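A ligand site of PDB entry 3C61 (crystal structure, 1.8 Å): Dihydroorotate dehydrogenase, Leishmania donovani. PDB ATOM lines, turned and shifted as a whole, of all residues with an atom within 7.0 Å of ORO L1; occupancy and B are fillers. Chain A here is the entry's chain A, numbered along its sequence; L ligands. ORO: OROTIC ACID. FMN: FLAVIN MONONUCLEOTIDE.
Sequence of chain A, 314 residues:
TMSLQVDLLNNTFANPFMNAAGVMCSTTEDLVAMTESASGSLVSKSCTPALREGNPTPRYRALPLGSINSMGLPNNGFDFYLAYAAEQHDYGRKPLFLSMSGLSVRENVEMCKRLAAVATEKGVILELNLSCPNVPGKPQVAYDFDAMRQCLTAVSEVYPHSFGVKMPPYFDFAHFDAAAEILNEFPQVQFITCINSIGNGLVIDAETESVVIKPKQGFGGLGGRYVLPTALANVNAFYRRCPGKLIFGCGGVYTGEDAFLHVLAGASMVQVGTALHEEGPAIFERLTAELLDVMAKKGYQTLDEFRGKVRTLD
OG of Ser 197 sits at hydrogen-bond distance from OD1 of Asn 196, 3.5 Å away.
OD1 of Asn 129 is in hydrogen-bond range of OG of Ser 131.
The side-chain hydroxyl (OG) of Ser 131 lies within hydrogen-bond range of the side-chain amide nitrogen (ND2) of Asn 196 (2.8 Å).
The backbone carbonyl oxygen of Asn 69 is in hydrogen-bond range of the backbone NH of Gly 221, at 2.7 Å.
The backbone NH (N) of Asn 134 sits close to the side-chain sulfur (SG) of Cys 132 (3.7 Å).
The backbone NH of Gly 72 sits close to the side-chain amide nitrogen of Asn 55 (3.4 Å).
The side-chain amide oxygen (OD1) of Asn 134 sits close to the side-chain amide oxygen (OD1) of Asn 69 (3.3 Å).
OD1 of Asn 69 lies within hydrogen-bond range of N of Met 71, 3.1 Å away.
The backbone NH of Leu 73 lies within hydrogen-bond range of an oxygen (O71) of ORO L1, at 3.0 Å.
The backbone NH of Gly 72 sits at hydrogen-bond distance from an oxygen (O72) of ORO L1 (2.7 Å).
O2 of ORO L1 lies within hydrogen-bond range of ND2 of Asn 69 (3.2 Å).
ND2 of Asn 129 sits at hydrogen-bond distance from O2 of FMN L2.
The side-chain amino group (NZ) of Lys 166 sits at hydrogen-bond distance from an oxygen (O2) of FMN L2, at 2.7 Å.
ND2 of Asn 196 sits at hydrogen-bond distance from O2 of FMN L2, at 3.3 Å.
The side-chain amino group of Lys 45 lies close to an oxygen (O4) of FMN L2, 3.4 Å away.
OG of Ser 197 sits at hydrogen-bond distance from O2 of ORO L1, at 3.0 Å.
An oxygen (O4) of ORO L1 is in hydrogen-bond range of the side-chain amide nitrogen of Asn 129.
The side-chain amide oxygen of Asn 196 is in hydrogen-bond range of a nitrogen (N3) of ORO L1, 2.7 Å away.
OD1 of Asn 134 sits at hydrogen-bond distance from N1 of ORO L1 (2.7 Å).
O2' of FMN L2 sits at hydrogen-bond distance from O of Ala 21 (3.0 Å).
The side-chain hydroxyl (OG) of Ser 46 is in hydrogen-bond range of a nitrogen (N3) of FMN L2 (2.4 Å).
Residues that only touch ORO L1: Cys 132 (3.2 Å), Pro 133 (3.3 Å), Met 71 (3.5 Å) and Pro 74 (3.8 Å).
The nearest printed residue that does not touch ORO L1 is Lys 45 (4.1 Å).
A nitrogen (N3) of FMN L2 lies close to an oxygen (O4) of ORO L1.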
ATOM      1  N   ALA A  21      -1.377  25.017 -22.152  1.00  0.00           N
ATOM      2  CA  ALA A  21      -1.856  25.428 -20.866  1.00  0.00           C
ATOM      3  C   ALA A  21      -0.868  26.474 -20.343  1.00  0.00           C
ATOM      4  O   ALA A  21       0.323  26.415 -20.602  1.00  0.00           O
ATOM      5  CB  ALA A  21      -1.960  24.222 -19.927  1.00  0.00           C
ATOM      6  N   GLY A  22      -1.346  27.457 -19.649  1.00  0.00           N
ATOM      7  CA  GLY A  22      -0.411  28.511 -19.219  1.00  0.00           C
ATOM      8  C   GLY A  22      -0.372  29.728 -20.118  1.00  0.00           C
ATOM      9  O   GLY A  22       0.036  30.799 -19.657  1.00  0.00           O
ATOM     10  N   LYS A  45      -5.855  27.353 -17.772  1.00  0.00           N
ATOM     11  CA  LYS A  45      -4.628  27.485 -17.000  1.00  0.00           C
ATOM     12  C   LYS A  45      -4.480  26.382 -15.960  1.00  0.00           C
ATOM     13  O   LYS A  45      -5.417  26.126 -15.186  1.00  0.00           O
ATOM     14  CB  LYS A  45      -4.623  28.849 -16.282  1.00  0.00           C
ATOM     15  CG  LYS A  45      -3.475  29.107 -15.319  1.00  0.00           C
ATOM     16  CD  LYS A  45      -2.141  29.143 -16.067  1.00  0.00           C
ATOM     17  CE  LYS A  45      -0.921  29.222 -15.133  1.00  0.00           C
ATOM     18  NZ  LYS A  45      -0.917  28.257 -13.973  1.00  0.00           N
ATOM     19  N   SER A  46      -3.306  25.745 -15.914  1.00  0.00           N
ATOM     20  CA  SER A  46      -3.000  24.752 -14.886  1.00  0.00           C
ATOM     21  C   SER A  46      -3.369  25.293 -13.492  1.00  0.00           C
ATOM     22  O   SER A  46      -2.834  26.322 -13.046  1.00  0.00           O
ATOM     23  CB  SER A  46      -1.530  24.332 -14.940  1.00  0.00           C
ATOM     24  OG  SER A  46      -1.260  23.758 -16.207  1.00  0.00           O
ATOM     25  N   ASN A  55       4.904  33.821  -9.210  1.00  0.00           N
ATOM     26  CA  ASN A  55       6.231  34.281  -8.761  1.00  0.00           C
ATOM     27  C   ASN A  55       6.361  35.784  -9.011  1.00  0.00           C
ATOM     28  O   ASN A  55       5.560  36.372  -9.742  1.00  0.00           O
ATOM     29  CB  ASN A  55       7.358  33.507  -9.493  1.00  0.00           C
ATOM     30  CG  ASN A  55       7.481  32.043  -9.065  1.00  0.00           C
ATOM     31  OD1 ASN A  55       7.152  31.653  -7.943  1.00  0.00           O
ATOM     32  ND2 ASN A  55       8.002  31.227  -9.978  1.00  0.00           N
ATOM     33  N   ASN A  69      10.454  31.476 -19.000  1.00  0.00           N
ATOM     34  CA  ASN A  69       9.512  31.902 -17.957  1.00  0.00           C
ATOM     35  C   ASN A  69       9.706  31.162 -16.654  1.00  0.00           C
ATOM     36  O   ASN A  69      10.148  30.004 -16.639  1.00  0.00           O
ATOM     37  CB  ASN A  69       8.071  31.768 -18.443  1.00  0.00           C
ATOM     38  CG  ASN A  69       7.477  30.385 -18.140  1.00  0.00           C
ATOM     39  OD1 ASN A  69       7.031  30.122 -16.999  1.00  0.00           O
ATOM     40  ND2 ASN A  69       7.509  29.497 -19.120  1.00  0.00           N
ATOM     41  N   SER A  70       9.347  31.840 -15.563  1.00  0.00           N
ATOM     42  CA  SER A  70       9.156  31.183 -14.280  1.00  0.00           C
ATOM     43  C   SER A  70       7.907  31.771 -13.652  1.00  0.00           C
ATOM     44  O   SER A  70       7.985  32.517 -12.681  1.00  0.00           O
ATOM     45  CB  SER A  70      10.362  31.404 -13.382  1.00  0.00           C
ATOM     46  OG  SER A  70      10.213  30.729 -12.143  1.00  0.00           O
ATOM     47  N   MET A  71       6.762  31.495 -14.255  1.00  0.00           N
ATOM     48  CA  MET A  71       5.500  32.100 -13.801  1.00  0.00           C
ATOM     49  C   MET A  71       5.163  31.672 -12.357  1.00  0.00           C
ATOM     50  O   MET A  71       4.654  32.485 -11.577  1.00  0.00           O
ATOM     51  CB  MET A  71       4.322  31.745 -14.719  1.00  0.00           C
ATOM     52  CG  MET A  71       4.521  31.970 -16.208  1.00  0.00           C
ATOM     53  SD  MET A  71       4.917  33.666 -16.689  1.00  0.00           S
ATOM     54  CE  MET A  71       3.428  34.532 -16.220  1.00  0.00           C
ATOM     55  N   GLY A  72       5.419  30.403 -12.016  1.00  0.00           N
ATOM     56  CA  GLY A  72       5.049  29.855 -10.680  1.00  0.00           C
ATOM     57  C   GLY A  72       3.574  29.477 -10.463  1.00  0.00           C
ATOM     58  O   GLY A  72       2.984  29.714  -9.391  1.00  0.00           O
ATOM     59  N   LEU A  73       2.966  28.878 -11.472  1.00  0.00           N
ATOM     60  CA  LEU A  73       1.529  28.526 -11.447  1.00  0.00           C
ATOM     61  C   LEU A  73       0.563  29.637 -10.971  1.00  0.00           C
ATOM     62  O   LEU A  73      -0.330  29.375 -10.164  1.00  0.00           O
ATOM     63  CB  LEU A  73       1.313  27.225 -10.639  1.00  0.00           C
ATOM     64  CG  LEU A  73       1.814  25.918 -11.286  1.00  0.00           C
ATOM     65  CD1 LEU A  73       1.581  24.730 -10.350  1.00  0.00           C
ATOM     66  CD2 LEU A  73       1.151  25.676 -12.655  1.00  0.00           C
ATOM     67  N   PRO A  74       0.707  30.869 -11.500  1.00  0.00           N
ATOM     68  CA  PRO A  74      -0.335  31.862 -11.248  1.00  0.00           C
ATOM     69  C   PRO A  74      -1.644  31.415 -11.840  1.00  0.00           C
ATOM     70  O   PRO A  74      -1.728  31.095 -13.019  1.00  0.00           O
ATOM     71  CB  PRO A  74       0.166  33.101 -11.997  1.00  0.00           C
ATOM     72  CG  PRO A  74       1.013  32.593 -13.025  1.00  0.00           C
ATOM     73  CD  PRO A  74       1.681  31.371 -12.486  1.00  0.00           C
ATOM     74  N   SER A  99      -6.652  21.953 -17.337  1.00  0.00           N
ATOM     75  CA  SER A  99      -5.339  21.539 -16.869  1.00  0.00           C
ATOM     76  C   SER A  99      -5.259  21.644 -15.352  1.00  0.00           C
ATOM     77  O   SER A  99      -5.604  22.657 -14.772  1.00  0.00           O
ATOM     78  CB  SER A  99      -4.217  22.406 -17.477  1.00  0.00           C
ATOM     79  OG  SER A  99      -2.986  22.032 -16.895  1.00  0.00           O
ATOM     80  N   SER A 101      -2.791  21.085 -11.867  1.00  0.00           N
ATOM     81  CA  SER A 101      -1.429  20.986 -11.384  1.00  0.00           C
ATOM     82  C   SER A 101      -1.385  21.131  -9.862  1.00  0.00           C
ATOM     83  O   SER A 101      -0.773  22.049  -9.337  1.00  0.00           O
ATOM     84  CB  SER A 101      -0.559  22.027 -12.089  1.00  0.00           C
ATOM     85  OG  SER A 101       0.821  21.706 -11.959  1.00  0.00           O
ATOM     86  N   ASN A 129      -1.224  17.809 -15.194  1.00  0.00           N
ATOM     87  CA  ASN A 129       0.145  18.310 -15.373  1.00  0.00           C
ATOM     88  C   ASN A 129       1.134  17.630 -14.434  1.00  0.00           C
ATOM     89  O   ASN A 129       1.132  17.857 -13.216  1.00  0.00           O
ATOM     90  CB  ASN A 129       0.147  19.839 -15.190  1.00  0.00           C
ATOM     91  CG  ASN A 129       1.468  20.471 -15.536  1.00  0.00           C
ATOM     92  OD1 ASN A 129       2.394  19.788 -15.984  1.00  0.00           O
ATOM     93  ND2 ASN A 129       1.572  21.795 -15.346  1.00  0.00           N
ATOM     94  N   SER A 131       4.452  17.989 -14.880  1.00  0.00           N
ATOM     95  CA  SER A 131       5.712  18.533 -15.417  1.00  0.00           C
ATOM     96  C   SER A 131       6.019  19.992 -15.177  1.00  0.00           C
ATOM     97  O   SER A 131       6.889  20.543 -15.854  1.00  0.00           O
ATOM     98  CB  SER A 131       5.744  18.309 -16.924  1.00  0.00           C
ATOM     99  OG  SER A 131       4.589  18.793 -17.582  1.00  0.00           O
ATOM    100  N   CYS A 132       5.327  20.628 -14.232  1.00  0.00           N
ATOM    101  CA  CYS A 132       5.607  22.058 -13.957  1.00  0.00           C
ATOM    102  C   CYS A 132       7.007  22.268 -13.337  1.00  0.00           C
ATOM    103  O   CYS A 132       7.240  21.830 -12.198  1.00  0.00           O
ATOM    104  CB  CYS A 132       4.566  22.670 -13.027  1.00  0.00           C
ATOM    105  SG  CYS A 132       4.972  24.392 -12.632  1.00  0.00           S
ATOM    106  N   PRO A 133       7.917  22.956 -14.069  1.00  0.00           N
ATOM    107  CA  PRO A 133       9.299  23.124 -13.583  1.00  0.00           C
ATOM    108  C   PRO A 133       9.616  24.470 -12.859  1.00  0.00           C
ATOM    109  O   PRO A 133      10.800  24.782 -12.661  1.00  0.00           O
ATOM    110  CB  PRO A 133      10.129  23.027 -14.886  1.00  0.00           C
ATOM    111  CG  PRO A 133       9.202  23.615 -15.973  1.00  0.00           C
ATOM    112  CD  PRO A 133       7.760  23.542 -15.420  1.00  0.00           C
ATOM    113  N   ASN A 134       8.588  25.222 -12.455  1.00  0.00           N
ATOM    114  CA  ASN A 134       8.784  26.614 -11.956  1.00  0.00           C
ATOM    115  C   ASN A 134       8.253  26.940 -10.540  1.00  0.00           C
ATOM    116  O   ASN A 134       8.378  28.091 -10.089  1.00  0.00           O
ATOM    117  CB  ASN A 134       8.185  27.619 -12.950  1.00  0.00           C
ATOM    118  CG  ASN A 134       8.835  27.534 -14.332  1.00  0.00           C
ATOM    119  OD1 ASN A 134       8.138  27.538 -15.356  1.00  0.00           O
ATOM    120  ND2 ASN A 134      10.167  27.420 -14.368  1.00  0.00           N
ATOM    121  N   VAL A 135       7.667  25.960  -9.858  1.00  0.00           N
ATOM    122  CA  VAL A 135       7.287  26.148  -8.459  1.00  0.00           C
ATOM    123  C   VAL A 135       8.526  25.812  -7.622  1.00  0.00           C
ATOM    124  O   VAL A 135       8.997  24.661  -7.636  1.00  0.00           O
ATOM    125  CB  VAL A 135       6.099  25.264  -8.048  1.00  0.00           C
ATOM    126  CG1 VAL A 135       5.809  25.404  -6.561  1.00  0.00           C
ATOM    127  CG2 VAL A 135       4.869  25.656  -8.871  1.00  0.00           C
ATOM    128  N   LYS A 166       0.231  15.813 -19.115  1.00  0.00           N
ATOM    129  CA  LYS A 166       1.235  16.727 -19.676  1.00  0.00           C
ATOM    130  C   LYS A 166       2.600  16.364 -19.120  1.00  0.00           C
ATOM    131  O   LYS A 166       2.835  16.401 -17.896  1.00  0.00           O
ATOM    132  CB  LYS A 166       0.888  18.166 -19.320  1.00  0.00           C
ATOM    133  CG  LYS A 166       1.870  19.226 -19.800  1.00  0.00           C
ATOM    134  CD  LYS A 166       1.712  19.530 -21.262  1.00  0.00           C
ATOM    135  CE  LYS A 166       2.393  20.846 -21.660  1.00  0.00           C
ATOM    136  NZ  LYS A 166       1.657  22.104 -21.216  1.00  0.00           N
ATOM    137  N   ASN A 196       6.006  19.900 -21.994  1.00  0.00           N
ATOM    138  CA  ASN A 196       6.088  21.106 -21.209  1.00  0.00           C
ATOM    139  C   ASN A 196       7.466  21.696 -21.591  1.00  0.00           C
ATOM    140  O   ASN A 196       8.180  21.154 -22.436  1.00  0.00           O
ATOM    141  CB  ASN A 196       5.978  20.768 -19.733  1.00  0.00           C
ATOM    142  CG  ASN A 196       5.355  21.881 -18.914  1.00  0.00           C
ATOM    143  OD1 ASN A 196       5.836  23.003 -18.932  1.00  0.00           O
ATOM    144  ND2 ASN A 196       4.313  21.569 -18.151  1.00  0.00           N
ATOM    145  N   SER A 197       7.810  22.790 -21.013  1.00  0.00           N
ATOM    146  CA  SER A 197       9.018  23.503 -21.410  1.00  0.00           C
ATOM    147  C   SER A 197      10.251  22.642 -21.161  1.00  0.00           C
ATOM    148  O   SER A 197      10.190  21.609 -20.470  1.00  0.00           O
ATOM    149  CB  SER A 197       9.111  24.789 -20.593  1.00  0.00           C
ATOM    150  OG  SER A 197       8.966  24.493 -19.224  1.00  0.00           O
ATOM    151  N   ILE A 198      11.373  23.058 -21.740  1.00  0.00           N
ATOM    152  CA  ILE A 198      12.634  22.496 -21.356  1.00  0.00           C
ATOM    153  C   ILE A 198      13.007  23.227 -20.075  1.00  0.00           C
ATOM    154  O   ILE A 198      13.228  24.467 -20.069  1.00  0.00           O
ATOM    155  CB  ILE A 198      13.728  22.630 -22.447  1.00  0.00           C
ATOM    156  CG1 ILE A 198      13.356  21.834 -23.693  1.00  0.00           C
ATOM    157  CG2 ILE A 198      15.083  22.166 -21.917  1.00  0.00           C
ATOM    158  CD1 ILE A 198      14.346  21.932 -24.818  1.00  0.00           C
ATOM    159  N   GLY A 220      14.570  29.303 -15.597  1.00  0.00           N
ATOM    160  CA  GLY A 220      13.188  29.168 -16.011  1.00  0.00           C
ATOM    161  C   GLY A 220      13.007  28.230 -17.185  1.00  0.00           C
ATOM    162  O   GLY A 220      13.963  27.800 -17.800  1.00  0.00           O
ATOM    163  N   GLY A 221      11.752  27.942 -17.480  1.00  0.00           N
ATOM    164  CA  GLY A 221      11.418  27.012 -18.549  1.00  0.00           C
ATOM    165  C   GLY A 221      11.549  27.668 -19.904  1.00  0.00           C
ATOM    166  O   GLY A 221      11.068  28.804 -20.111  1.00  0.00           O
ATOM    167  N   LEU A 222      12.167  26.949 -20.824  1.00  0.00           N
ATOM    168  CA  LEU A 222      12.313  27.371 -22.209  1.00  0.00           C
ATOM    169  C   LEU A 222      11.186  26.900 -23.106  1.00  0.00           C
ATOM    170  O   LEU A 222      10.738  25.747 -23.023  1.00  0.00           O
ATOM    171  CB  LEU A 222      13.643  26.856 -22.794  1.00  0.00           C
ATOM    172  CG  LEU A 222      14.944  27.210 -22.081  1.00  0.00           C
ATOM    173  CD1 LEU A 222      16.103  26.456 -22.765  1.00  0.00           C
ATOM    174  CD2 LEU A 222      15.198  28.716 -22.029  1.00  0.00           C
HETATM  175  N1  ORO L   1       5.675  27.164 -16.360  1.00  0.00           N
HETATM  176  C2  ORO L   1       6.029  26.227 -17.262  1.00  0.00           C
HETATM  177  O2  ORO L   1       6.971  26.502 -18.117  1.00  0.00           O
HETATM  178  N3  ORO L   1       5.373  25.026 -17.228  1.00  0.00           N
HETATM  179  C4  ORO L   1       4.390  24.742 -16.293  1.00  0.00           C
HETATM  180  O4  ORO L   1       3.731  23.671 -16.176  1.00  0.00           O
HETATM  181  C5  ORO L   1       4.055  25.714 -15.405  1.00  0.00           C
HETATM  182  C6  ORO L   1       4.709  26.928 -15.456  1.00  0.00           C
HETATM  183  C7  ORO L   1       4.319  27.933 -14.448  1.00  0.00           C
HETATM  184  O71 ORO L   1       3.197  28.442 -14.415  1.00  0.00           O
HETATM  185  O72 ORO L   1       5.185  28.241 -13.638  1.00  0.00           O
HETATM  186  N1  FMN L   2       2.411  24.243 -19.138  1.00  0.00           N
HETATM  187  C2  FMN L   2       1.437  23.654 -18.383  1.00  0.00           C
HETATM  188  O2  FMN L   2       1.178  22.472 -18.609  1.00  0.00           O
HETATM  189  N3  FMN L   2       0.776  24.362 -17.407  1.00  0.00           N
HETATM  190  C4  FMN L   2       1.073  25.690 -17.183  1.00  0.00           C
HETATM  191  O4  FMN L   2       0.250  26.393 -16.571  1.00  0.00           O
HETATM  192  C4A FMN L   2       2.083  26.305 -17.936  1.00  0.00           C
HETATM  193  N5  FMN L   2       2.428  27.626 -17.738  1.00  0.00           N
HETATM  194  C5A FMN L   2       3.118  28.271 -18.770  1.00  0.00           C
HETATM  195  C6  FMN L   2       3.154  29.665 -18.817  1.00  0.00           C
HETATM  196  C7  FMN L   2       3.843  30.310 -19.849  1.00  0.00           C
HETATM  197  C7M FMN L   2       3.902  31.805 -19.938  1.00  0.00           C
HETATM  198  C8  FMN L   2       4.504  29.565 -20.826  1.00  0.00           C
HETATM  199  C8M FMN L   2       5.235  30.250 -21.949  1.00  0.00           C
HETATM  200  C9  FMN L   2       4.457  28.183 -20.786  1.00  0.00           C
HETATM  201  C9A FMN L   2       3.786  27.521 -19.751  1.00  0.00           C
HETATM  202  N10 FMN L   2       3.707  26.128 -19.706  1.00  0.00           N
HETATM  203  C10 FMN L   2       2.675  25.587 -18.986  1.00  0.00           C
HETATM  204  C1' FMN L   2       4.317  25.266 -20.778  1.00  0.00           C
HETATM  205  C2' FMN L   2       3.535  25.346 -22.096  1.00  0.00           C
HETATM  206  O2' FMN L   2       2.299  24.692 -21.968  1.00  0.00           O
HETATM  207  C3' FMN L   2       4.256  24.678 -23.247  1.00  0.00           C
HETATM  208  O3' FMN L   2       4.391  23.319 -22.880  1.00  0.00           O
HETATM  209  C4' FMN L   2       5.643  25.259 -23.580  1.00  0.00           C
HETATM  210  O4' FMN L   2       5.708  26.678 -23.456  1.00  0.00           O
HETATM  211  C5' FMN L   2       6.165  24.828 -24.952  1.00  0.00           C
HETATM  212  O5' FMN L   2       5.390  25.301 -26.039  1.00  0.00           O
HETATM  213  P   FMN L   2       5.916  26.509 -26.978  1.00  0.00           P
HETATM  214  O1P FMN L   2       7.273  26.110 -27.503  1.00  0.00           O
HETATM  215  O2P FMN L   2       6.034  27.655 -25.998  1.00  0.00           O
HETATM  216  O3P FMN L   2       4.872  26.652 -28.031  1.00  0.00           O
